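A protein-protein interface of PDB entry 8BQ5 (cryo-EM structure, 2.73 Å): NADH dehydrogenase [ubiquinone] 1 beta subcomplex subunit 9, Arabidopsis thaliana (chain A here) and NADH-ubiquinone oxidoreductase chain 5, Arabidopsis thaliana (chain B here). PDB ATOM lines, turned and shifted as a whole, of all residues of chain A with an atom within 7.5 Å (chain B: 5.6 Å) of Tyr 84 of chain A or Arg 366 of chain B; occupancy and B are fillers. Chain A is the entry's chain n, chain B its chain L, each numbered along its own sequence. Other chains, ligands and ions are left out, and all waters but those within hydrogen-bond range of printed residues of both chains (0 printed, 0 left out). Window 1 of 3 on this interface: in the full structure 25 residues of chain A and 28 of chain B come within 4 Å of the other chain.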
ATOM      1  N   LYS A  29     -14.957   4.940 -14.288  1.00  0.00           N
ATOM      2  CA  LYS A  29     -13.543   5.218 -14.515  1.00  0.00           C
ATOM      3  C   LYS A  29     -12.658   4.354 -13.629  1.00  0.00           C
ATOM      4  O   LYS A  29     -11.561   3.963 -14.043  1.00  0.00           O
ATOM      5  CB  LYS A  29     -13.237   6.695 -14.281  1.00  0.00           C
ATOM      6  CG  LYS A  29     -13.648   7.606 -15.422  1.00  0.00           C
ATOM      7  CD  LYS A  29     -13.853   9.026 -14.930  1.00  0.00           C
ATOM      8  CE  LYS A  29     -13.826  10.015 -16.079  1.00  0.00           C
ATOM      9  NZ  LYS A  29     -12.690  10.968 -15.963  1.00  0.00           N
ATOM     10  N   ASP A  30     -13.147   4.058 -12.422  1.00  0.00           N
ATOM     11  CA  ASP A  30     -12.404   3.146 -11.521  1.00  0.00           C
ATOM     12  C   ASP A  30     -12.355   1.749 -12.141  1.00  0.00           C
ATOM     13  O   ASP A  30     -11.360   1.049 -11.908  1.00  0.00           O
ATOM     14  CB  ASP A  30     -13.053   3.072 -10.145  1.00  0.00           C
ATOM     15  CG  ASP A  30     -12.107   2.533  -9.095  1.00  0.00           C
ATOM     16  OD1 ASP A  30     -12.434   1.502  -8.482  1.00  0.00           O
ATOM     17  OD2 ASP A  30     -11.040   3.144  -8.924  1.00  0.00           O
ATOM     18  N   LEU A  32     -12.026   0.840 -15.293  1.00  0.00           N
ATOM     19  CA  LEU A  32     -10.979   0.701 -16.297  1.00  0.00           C
ATOM     20  C   LEU A  32      -9.594   0.717 -15.655  1.00  0.00           C
ATOM     21  O   LEU A  32      -8.642   0.159 -16.212  1.00  0.00           O
ATOM     22  CB  LEU A  32     -11.120   1.804 -17.347  1.00  0.00           C
ATOM     23  CG  LEU A  32     -10.149   1.799 -18.527  1.00  0.00           C
ATOM     24  CD1 LEU A  32     -10.166   0.450 -19.222  1.00  0.00           C
ATOM     25  CD2 LEU A  32     -10.520   2.896 -19.503  1.00  0.00           C
ATOM     26  N   ASN A  33      -9.467   1.343 -14.481  1.00  0.00           N
ATOM     27  CA  ASN A  33      -8.194   1.322 -13.764  1.00  0.00           C
ATOM     28  C   ASN A  33      -7.829  -0.089 -13.328  1.00  0.00           C
ATOM     29  O   ASN A  33      -6.657  -0.481 -13.381  1.00  0.00           O
ATOM     30  CB  ASN A  33      -8.252   2.250 -12.550  1.00  0.00           C
ATOM     31  CG  ASN A  33      -8.271   3.712 -12.932  1.00  0.00           C
ATOM     32  OD1 ASN A  33      -7.505   4.150 -13.791  1.00  0.00           O
ATOM     33  ND2 ASN A  33      -9.140   4.480 -12.289  1.00  0.00           N
ATOM     34  N   TRP A  34      -8.824  -0.851 -12.877  1.00  0.00           N
ATOM     35  CA  TRP A  34      -8.583  -2.250 -12.439  1.00  0.00           C
ATOM     36  C   TRP A  34      -8.410  -3.196 -13.633  1.00  0.00           C
ATOM     37  O   TRP A  34      -7.571  -4.101 -13.516  1.00  0.00           O
ATOM     38  CB  TRP A  34      -9.733  -2.716 -11.546  1.00  0.00           C
ATOM     39  CG  TRP A  34      -9.744  -2.158 -10.157  1.00  0.00           C
ATOM     40  CD1 TRP A  34     -10.623  -1.248  -9.649  1.00  0.00           C
ATOM     41  CD2 TRP A  34      -8.862  -2.508  -9.076  1.00  0.00           C
ATOM     42  NE1 TRP A  34     -10.340  -0.995  -8.336  1.00  0.00           N
ATOM     43  CE2 TRP A  34      -9.265  -1.750  -7.956  1.00  0.00           C
ATOM     44  CE3 TRP A  34      -7.766  -3.368  -8.948  1.00  0.00           C
ATOM     45  CZ2 TRP A  34      -8.612  -1.834  -6.727  1.00  0.00           C
ATOM     46  CZ3 TRP A  34      -7.118  -3.443  -7.736  1.00  0.00           C
ATOM     47  CH2 TRP A  34      -7.540  -2.690  -6.641  1.00  0.00           C
ATOM     48  N   ALA A  35      -9.116  -2.974 -14.746  1.00  0.00           N
ATOM     49  CA  ALA A  35      -9.136  -3.900 -15.872  1.00  0.00           C
ATOM     50  C   ALA A  35      -8.043  -3.635 -16.895  1.00  0.00           C
ATOM     51  O   ALA A  35      -7.586  -4.572 -17.557  1.00  0.00           O
ATOM     52  CB  ALA A  35     -10.500  -3.853 -16.565  1.00  0.00           C
ATOM     53  N   VAL A  36      -7.632  -2.375 -17.052  1.00  0.00           N
ATOM     54  CA  VAL A  36      -6.532  -1.980 -17.929  1.00  0.00           C
ATOM     55  C   VAL A  36      -6.880  -2.268 -19.384  1.00  0.00           C
ATOM     56  O   VAL A  36      -7.088  -1.343 -20.176  1.00  0.00           O
ATOM     57  CB  VAL A  36      -5.219  -2.676 -17.525  1.00  0.00           C
ATOM     58  CG1 VAL A  36      -4.090  -2.257 -18.450  1.00  0.00           C
ATOM     59  CG2 VAL A  36      -4.881  -2.367 -16.077  1.00  0.00           C
ATOM     60  N   HIS A  37      -6.941  -3.548 -19.745  1.00  0.00           N
ATOM     61  CA  HIS A  37      -7.199  -3.940 -21.124  1.00  0.00           C
ATOM     62  C   HIS A  37      -8.612  -3.557 -21.541  1.00  0.00           C
ATOM     63  O   HIS A  37      -9.541  -3.572 -20.729  1.00  0.00           O
ATOM     64  CB  HIS A  37      -6.997  -5.444 -21.296  1.00  0.00           C
ATOM     65  CG  HIS A  37      -5.620  -5.907 -20.947  1.00  0.00           C
ATOM     66  ND1 HIS A  37      -4.500  -5.132 -21.154  1.00  0.00           N
ATOM     67  CD2 HIS A  37      -5.182  -7.059 -20.390  1.00  0.00           C
ATOM     68  CE1 HIS A  37      -3.430  -5.791 -20.744  1.00  0.00           C
ATOM     69  NE2 HIS A  37      -3.818  -6.962 -20.275  1.00  0.00           N
ATOM     70  N   ARG A  38      -8.765  -3.214 -22.821  1.00  0.00           N
ATOM     71  CA  ARG A  38     -10.066  -2.792 -23.329  1.00  0.00           C
ATOM     72  C   ARG A  38     -11.095  -3.910 -23.222  1.00  0.00           C
ATOM     73  O   ARG A  38     -12.218  -3.697 -22.751  1.00  0.00           O
ATOM     74  CB  ARG A  38      -9.935  -2.332 -24.781  1.00  0.00           C
ATOM     75  CG  ARG A  38      -8.869  -1.283 -25.005  1.00  0.00           C
ATOM     76  CD  ARG A  38      -9.093  -0.094 -24.095  1.00  0.00           C
ATOM     77  NE  ARG A  38     -10.231   0.707 -24.522  1.00  0.00           N
ATOM     78  CZ  ARG A  38     -10.679   1.771 -23.873  1.00  0.00           C
ATOM     79  NH1 ARG A  38     -10.111   2.187 -22.754  1.00  0.00           N
ATOM     80  NH2 ARG A  38     -11.725   2.434 -24.358  1.00  0.00           N
ATOM     81  N   HIS A  80      -9.479   2.131  -6.917  1.00  0.00           N
ATOM     82  CA  HIS A  80      -8.084   1.760  -7.281  1.00  0.00           C
ATOM     83  C   HIS A  80      -7.095   2.671  -6.551  1.00  0.00           C
ATOM     84  O   HIS A  80      -7.262   3.898  -6.634  1.00  0.00           O
ATOM     85  CB  HIS A  80      -7.898   1.849  -8.797  1.00  0.00           C
ATOM     86  CG  HIS A  80      -6.728   1.080  -9.301  1.00  0.00           C
ATOM     87  ND1 HIS A  80      -5.436   1.531  -9.162  1.00  0.00           N
ATOM     88  CD2 HIS A  80      -6.650  -0.101  -9.942  1.00  0.00           C
ATOM     89  CE1 HIS A  80      -4.607   0.658  -9.694  1.00  0.00           C
ATOM     90  NE2 HIS A  80      -5.330  -0.351 -10.183  1.00  0.00           N
ATOM     91  N   PRO A  81      -6.077   2.125  -5.845  1.00  0.00           N
ATOM     92  CA  PRO A  81      -5.152   2.955  -5.057  1.00  0.00           C
ATOM     93  C   PRO A  81      -4.235   3.853  -5.902  1.00  0.00           C
ATOM     94  O   PRO A  81      -3.704   4.792  -5.343  1.00  0.00           O
ATOM     95  CB  PRO A  81      -4.350   1.907  -4.278  1.00  0.00           C
ATOM     96  CG  PRO A  81      -4.395   0.684  -5.144  1.00  0.00           C
ATOM     97  CD  PRO A  81      -5.792   0.695  -5.722  1.00  0.00           C
ATOM     98  N   ASP A  82      -4.099   3.575  -7.201  1.00  0.00           N
ATOM     99  CA  ASP A  82      -3.272   4.377  -8.104  1.00  0.00           C
ATOM    100  C   ASP A  82      -4.034   4.586  -9.406  1.00  0.00           C
ATOM    101  O   ASP A  82      -3.794   3.890 -10.403  1.00  0.00           O
ATOM    102  CB  ASP A  82      -1.918   3.707  -8.340  1.00  0.00           C
ATOM    103  CG  ASP A  82      -1.083   4.421  -9.384  1.00  0.00           C
ATOM    104  OD1 ASP A  82      -0.661   5.569  -9.134  1.00  0.00           O
ATOM    105  OD2 ASP A  82      -0.847   3.829 -10.459  1.00  0.00           O
ATOM    106  N   PRO A  83      -4.965   5.535  -9.433  1.00  0.00           N
ATOM    107  CA  PRO A  83      -5.762   5.751 -10.643  1.00  0.00           C
ATOM    108  C   PRO A  83      -4.968   6.443 -11.737  1.00  0.00           C
ATOM    109  O   PRO A  83      -3.980   7.135 -11.481  1.00  0.00           O
ATOM    110  CB  PRO A  83      -6.910   6.638 -10.154  1.00  0.00           C
ATOM    111  CG  PRO A  83      -6.305   7.413  -9.034  1.00  0.00           C
ATOM    112  CD  PRO A  83      -5.303   6.499  -8.370  1.00  0.00           C
ATOM    113  N   TYR A  84      -5.422   6.249 -12.971  1.00  0.00           N
ATOM    114  CA  TYR A  84      -4.829   6.948 -14.099  1.00  0.00           C
ATOM    115  C   TYR A  84      -5.304   8.394 -14.135  1.00  0.00           C
ATOM    116  O   TYR A  84      -6.472   8.688 -13.865  1.00  0.00           O
ATOM    117  CB  TYR A  84      -5.185   6.246 -15.409  1.00  0.00           C
ATOM    118  CG  TYR A  84      -4.829   7.055 -16.632  1.00  0.00           C
ATOM    119  CD1 TYR A  84      -3.534   7.058 -17.132  1.00  0.00           C
ATOM    120  CD2 TYR A  84      -5.784   7.823 -17.282  1.00  0.00           C
ATOM    121  CE1 TYR A  84      -3.202   7.804 -18.241  1.00  0.00           C
ATOM    122  CE2 TYR A  84      -5.462   8.571 -18.390  1.00  0.00           C
ATOM    123  CZ  TYR A  84      -4.172   8.558 -18.868  1.00  0.00           C
ATOM    124  OH  TYR A  84      -3.855   9.304 -19.977  1.00  0.00           O
ATOM    125  N   ILE A  85      -4.390   9.302 -14.471  1.00  0.00           N
ATOM    126  CA  ILE A  85      -4.702  10.716 -14.644  1.00  0.00           C
ATOM    127  C   ILE A  85      -4.030  11.197 -15.921  1.00  0.00           C
ATOM    128  O   ILE A  85      -2.859  10.885 -16.165  1.00  0.00           O
ATOM    129  CB  ILE A  85      -4.245  11.556 -13.434  1.00  0.00           C
ATOM    130  CG1 ILE A  85      -5.140  11.289 -12.228  1.00  0.00           C
ATOM    131  CG2 ILE A  85      -4.270  13.039 -13.763  1.00  0.00           C
ATOM    132  CD1 ILE A  85      -4.496  11.637 -10.908  1.00  0.00           C
ATOM    133  N   VAL A  86      -4.772  11.940 -16.737  1.00  0.00           N
ATOM    134  CA  VAL A  86      -4.201  12.536 -17.951  1.00  0.00           C
ATOM    135  C   VAL A  86      -3.053  13.460 -17.559  1.00  0.00           C
ATOM    136  O   VAL A  86      -3.184  14.228 -16.585  1.00  0.00           O
ATOM    137  CB  VAL A  86      -5.291  13.294 -18.734  1.00  0.00           C
ATOM    138  CG1 VAL A  86      -4.722  13.972 -19.965  1.00  0.00           C
ATOM    139  CG2 VAL A  86      -6.400  12.336 -19.136  1.00  0.00           C
ATOM    140  N   PRO A  87      -1.915  13.430 -18.264  1.00  0.00           N
ATOM    141  CA  PRO A  87      -0.700  14.086 -17.742  1.00  0.00           C
ATOM    142  C   PRO A  87      -0.856  15.558 -17.390  1.00  0.00           C
ATOM    143  O   PRO A  87      -0.293  15.994 -16.378  1.00  0.00           O
ATOM    144  CB  PRO A  87       0.307  13.894 -18.883  1.00  0.00           C
ATOM    145  CG  PRO A  87      -0.131  12.639 -19.546  1.00  0.00           C
ATOM    146  CD  PRO A  87      -1.629  12.624 -19.466  1.00  0.00           C
ATOM    147  N   GLY A  91      -2.848  16.638 -10.723  1.00  0.00           N
ATOM    148  CA  GLY A  91      -2.298  15.391 -10.246  1.00  0.00           C
ATOM    149  C   GLY A  91      -1.570  14.579 -11.294  1.00  0.00           C
ATOM    150  O   GLY A  91      -1.031  13.515 -10.965  1.00  0.00           O
ATOM    151  N   GLY A  92      -1.542  15.040 -12.546  1.00  0.00           N
ATOM    152  CA  GLY A  92      -0.824  14.339 -13.586  1.00  0.00           C
ATOM    153  C   GLY A  92       0.663  14.629 -13.558  1.00  0.00           C
ATOM    154  O   GLY A  92       1.139  15.540 -12.883  1.00  0.00           O
ATOM    155  N   ASN B 305       2.528   1.238 -12.124  1.00  0.00           N
ATOM    156  CA  ASN B 305       1.998   1.468 -13.460  1.00  0.00           C
ATOM    157  C   ASN B 305       2.796   2.490 -14.255  1.00  0.00           C
ATOM    158  O   ASN B 305       2.674   2.530 -15.484  1.00  0.00           O
ATOM    159  CB  ASN B 305       0.537   1.931 -13.372  1.00  0.00           C
ATOM    160  CG  ASN B 305      -0.350   0.921 -12.679  1.00  0.00           C
ATOM    161  OD1 ASN B 305      -0.963   1.218 -11.655  1.00  0.00           O
ATOM    162  ND2 ASN B 305      -0.424  -0.283 -13.233  1.00  0.00           N
ATOM    163  N   GLU B 362       3.205  10.564 -22.041  1.00  0.00           N
ATOM    164  CA  GLU B 362       2.412   9.539 -21.378  1.00  0.00           C
ATOM    165  C   GLU B 362       3.350   8.554 -20.691  1.00  0.00           C
ATOM    166  O   GLU B 362       4.256   8.002 -21.322  1.00  0.00           O
ATOM    167  CB  GLU B 362       1.516   8.824 -22.389  1.00  0.00           C
ATOM    168  CG  GLU B 362       0.635   7.729 -21.804  1.00  0.00           C
ATOM    169  CD  GLU B 362      -0.366   8.258 -20.796  1.00  0.00           C
ATOM    170  OE1 GLU B 362      -1.199   9.110 -21.171  1.00  0.00           O
ATOM    171  OE2 GLU B 362      -0.326   7.819 -19.629  1.00  0.00           O
ATOM    172  N   ASP B 364       1.970   6.205 -18.131  1.00  0.00           N
ATOM    173  CA  ASP B 364       1.207   5.107 -17.558  1.00  0.00           C
ATOM    174  C   ASP B 364       1.208   3.936 -18.533  1.00  0.00           C
ATOM    175  O   ASP B 364       0.840   4.095 -19.701  1.00  0.00           O
ATOM    176  CB  ASP B 364      -0.221   5.550 -17.242  1.00  0.00           C
ATOM    177  CG  ASP B 364      -0.810   4.809 -16.065  1.00  0.00           C
ATOM    178  OD1 ASP B 364      -1.295   3.678 -16.256  1.00  0.00           O
ATOM    179  OD2 ASP B 364      -0.788   5.357 -14.943  1.00  0.00           O
ATOM    180  N   MET B 365       1.482   2.732 -18.036  1.00  0.00           N
ATOM    181  CA  MET B 365       1.492   1.517 -18.903  1.00  0.00           C
ATOM    182  C   MET B 365       0.058   1.049 -19.184  1.00  0.00           C
ATOM    183  O   MET B 365      -0.116   0.266 -20.135  1.00  0.00           O
ATOM    184  CB  MET B 365       2.276   0.380 -18.244  1.00  0.00           C
ATOM    185  CG  MET B 365       3.743   0.706 -18.038  1.00  0.00           C
ATOM    186  SD  MET B 365       4.720  -0.716 -17.490  1.00  0.00           S
ATOM    187  CE  MET B 365       3.654  -1.380 -16.214  1.00  0.00           C
ATOM    188  N   ARG B 366      -0.921   1.519 -18.402  1.00  0.00           N
ATOM    189  CA  ARG B 366      -2.337   1.094 -18.567  1.00  0.00           C
ATOM    190  C   ARG B 366      -2.980   1.906 -19.693  1.00  0.00           C
ATOM    191  O   ARG B 366      -4.166   1.665 -19.974  1.00  0.00           O
ATOM    192  CB  ARG B 366      -3.113   1.262 -17.257  1.00  0.00           C
ATOM    193  CG  ARG B 366      -2.586   0.428 -16.101  1.00  0.00           C
ATOM    194  CD  ARG B 366      -3.300   0.820 -14.825  1.00  0.00           C
ATOM    195  NE  ARG B 366      -2.948   2.181 -14.452  1.00  0.00           N
ATOM    196  CZ  ARG B 366      -3.461   2.838 -13.423  1.00  0.00           C
ATOM    197  NH1 ARG B 366      -4.365   2.262 -12.653  1.00  0.00           N
ATOM    198  NH2 ARG B 366      -3.063   4.071 -13.168  1.00  0.00           N
ATOM    199  N   LYS B 367      -2.230   2.820 -20.306  1.00  0.00           N
ATOM    200  CA  LYS B 367      -2.729   3.616 -21.453  1.00  0.00           C
ATOM    201  C   LYS B 367      -1.666   3.590 -22.547  1.00  0.00           C
ATOM    202  O   LYS B 367      -1.434   4.644 -23.172  1.00  0.00           O
ATOM    203  CB  LYS B 367      -3.060   5.049 -21.023  1.00  0.00           C
ATOM    204  CG  LYS B 367      -4.329   5.190 -20.196  1.00  0.00           C
ATOM    205  CD  LYS B 367      -5.557   4.613 -20.860  1.00  0.00           C
ATOM    206  CE  LYS B 367      -6.803   4.779 -20.019  1.00  0.00           C
ATOM    207  NZ  LYS B 367      -6.595   4.292 -18.634  1.00  0.00           N
ATOM    208  N   MET B 368      -1.006   2.449 -22.733  1.00  0.00           N
ATOM    209  CA  MET B 368      -0.039   2.315 -23.847  1.00  0.00           C
ATOM    210  C   MET B 368      -0.466   1.108 -24.691  1.00  0.00           C
ATOM    211  O   MET B 368      -1.578   1.139 -25.214  1.00  0.00           O
ATOM    212  CB  MET B 368       1.389   2.144 -23.329  1.00  0.00           C
ATOM    213  CG  MET B 368       1.968   3.435 -22.792  1.00  0.00           C
ATOM    214  SD  MET B 368       3.602   3.235 -22.063  1.00  0.00           S
ATOM    215  CE  MET B 368       3.897   4.900 -21.475  1.00  0.00           C
ATOM    216  N   ASN B 447      -3.889  -0.162 -25.596  1.00  0.00           N
ATOM    217  CA  ASN B 447      -4.833   0.495 -24.705  1.00  0.00           C
ATOM    218  C   ASN B 447      -4.626   2.003 -24.705  1.00  0.00           C
ATOM    219  O   ASN B 447      -5.182   2.710 -23.859  1.00  0.00           O
ATOM    220  CB  ASN B 447      -4.712  -0.065 -23.290  1.00  0.00           C
ATOM    221  CG  ASN B 447      -5.029  -1.545 -23.224  1.00  0.00           C
ATOM    222  OD1 ASN B 447      -6.043  -1.998 -23.751  1.00  0.00           O
ATOM    223  ND2 ASN B 447      -4.157  -2.308 -22.578  1.00  0.00           N
ATOM    224  N   PHE B 449      -4.333   6.045 -26.387  1.00  0.00           N
ATOM    225  CA  PHE B 449      -5.296   6.986 -26.939  1.00  0.00           C
ATOM    226  C   PHE B 449      -5.035   7.215 -28.421  1.00  0.00           C
ATOM    227  O   PHE B 449      -3.898   7.102 -28.888  1.00  0.00           O
ATOM    228  CB  PHE B 449      -5.233   8.319 -26.195  1.00  0.00           C
ATOM    229  CG  PHE B 449      -5.839   8.281 -24.825  1.00  0.00           C
ATOM    230  CD1 PHE B 449      -7.200   8.451 -24.654  1.00  0.00           C
ATOM    231  CD2 PHE B 449      -5.047   8.082 -23.708  1.00  0.00           C
ATOM    232  CE1 PHE B 449      -7.761   8.424 -23.396  1.00  0.00           C
ATOM    233  CE2 PHE B 449      -5.603   8.053 -22.446  1.00  0.00           C
ATOM    234  CZ  PHE B 449      -6.961   8.224 -22.289  1.00  0.00           C
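A ring nitrogen (ND1) of His 37 of chain A sits at hydrogen-bond distance from the side-chain amide nitrogen of Asn 447 of chain B, 3.2 Å away.
OD1 of Asn 305 of chain B lies close to OD2 of Asp 82 of chain A (2.9 Å).
OD2 of Asp 82 of chain A is in salt-bridge range of NH2 of Arg 366 of chain B, 3.5 Å away.
The side-chain carboxylate (OE1) of Glu 362 of chain B lies within hydrogen-bond range of the side-chain hydroxyl (OH) of Tyr 84 of chain A (2.9 Å).
NH2 of Arg 366 of chain B lies close to N of Tyr 84 of chain A (3.2 Å).
The backbone NH of Arg 38 of chain A sits at hydrogen-bond distance from the side-chain amide oxygen of Asn 447 of chain B (3.1 Å).
The side-chain carboxylate (OE2) of Glu 362 of chain B is in hydrogen-bond range of the backbone NH (N) of Asp 364 of chain B (3.2 Å).
The backbone carbonyl oxygen (O) of Met 368 of chain B is in hydrogen-bond range of the backbone NH (N) of Asn 447 of chain B, 2.7 Å away.
A ring nitrogen (NE2) of His 80 of chain A sits close to the backbone carbonyl oxygen of Asn 33 of chain A (3.5 Å).
A ring nitrogen (ND1) of His 80 of chain A sits at hydrogen-bond distance from the backbone carbonyl oxygen (O) of Asp 82 of chain A.
The side-chain carboxylate of Asp 364 of chain B is in salt-bridge range of the guanidinium group of Arg 366 of chain B, 2.9 Å away.
The side-chain amide oxygen (OD1) of Asn 33 of chain A lies within hydrogen-bond range of the backbone NH (N) of Tyr 84 of chain A (3.1 Å).
Among the printed residues, merely in contact across the chains: Asn 33 of chain A with Arg 366 of chain B (3.6 Å), Val 36 of chain A with Arg 366 of chain B (3.6 Å), Val 36 of chain A with Asn 447 of chain B (3.7 Å), His 80 of chain A with Arg 366 of chain B (3.4 Å), Pro 83 of chain A with Arg 366 of chain B (3.4 Å), Tyr 84 of chain A with Asp 364 of chain B (3.6 Å), Tyr 84 of chain A with Lys 367 of chain B (3.5 Å), Tyr 84 of chain A with Phe 449 of chain B (3.3 Å) and Pro 87 of chain A with Glu 362 of chain B (3.9 Å).
Of the printed residues of chain B, Arg 38 of chain A touches Asn 447 (3.1 Å).
Of the printed residues of chain B, His 80 of chain A touches Arg 366 (3.4 Å).
Printed residues of chain B within 4 Å of Asp 82 of chain A: Asn 305 and Arg 366.
Tyr 84 of chain A touches five residues of chain B.
Of the printed residues of chain A, Arg 366 of chain B touches Asn 33 (3.6 Å), Val 36 (3.6 Å), His 80 (3.4 Å), Asp 82 (2.8 Å), Pro 83 (3.4 Å) and Tyr 84 (3.2 Å).
Printed residues of chain A within 4 Å of Lys 367 of chain B: Tyr 84 (3.5 Å).
The nearest printed residue of chain B that does not touch Tyr 84 of chain A is Met 365 of chain B (6.7 Å).
Hydrophobic or aromatic side chains of chain A that line the printed part of chain B: Val 36, His 37, His 80, Tyr 84 and Pro 87.
Of the 9 printed residues of chain B, 7 touch a printed residue of chain A.
Printed residues of chain B that touch a printed residue of chain A: Asn 305, Glu 362, Asp 364, Arg 366, Lys 367, Asn 447 and Phe 449.
Among the printed residues, Asp or Glu carboxylates within 4 Å of a Lys or Arg side-chain nitrogen of the other chain: Asp 82 of chain A with Arg 366 of chain B (3.5 Å).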
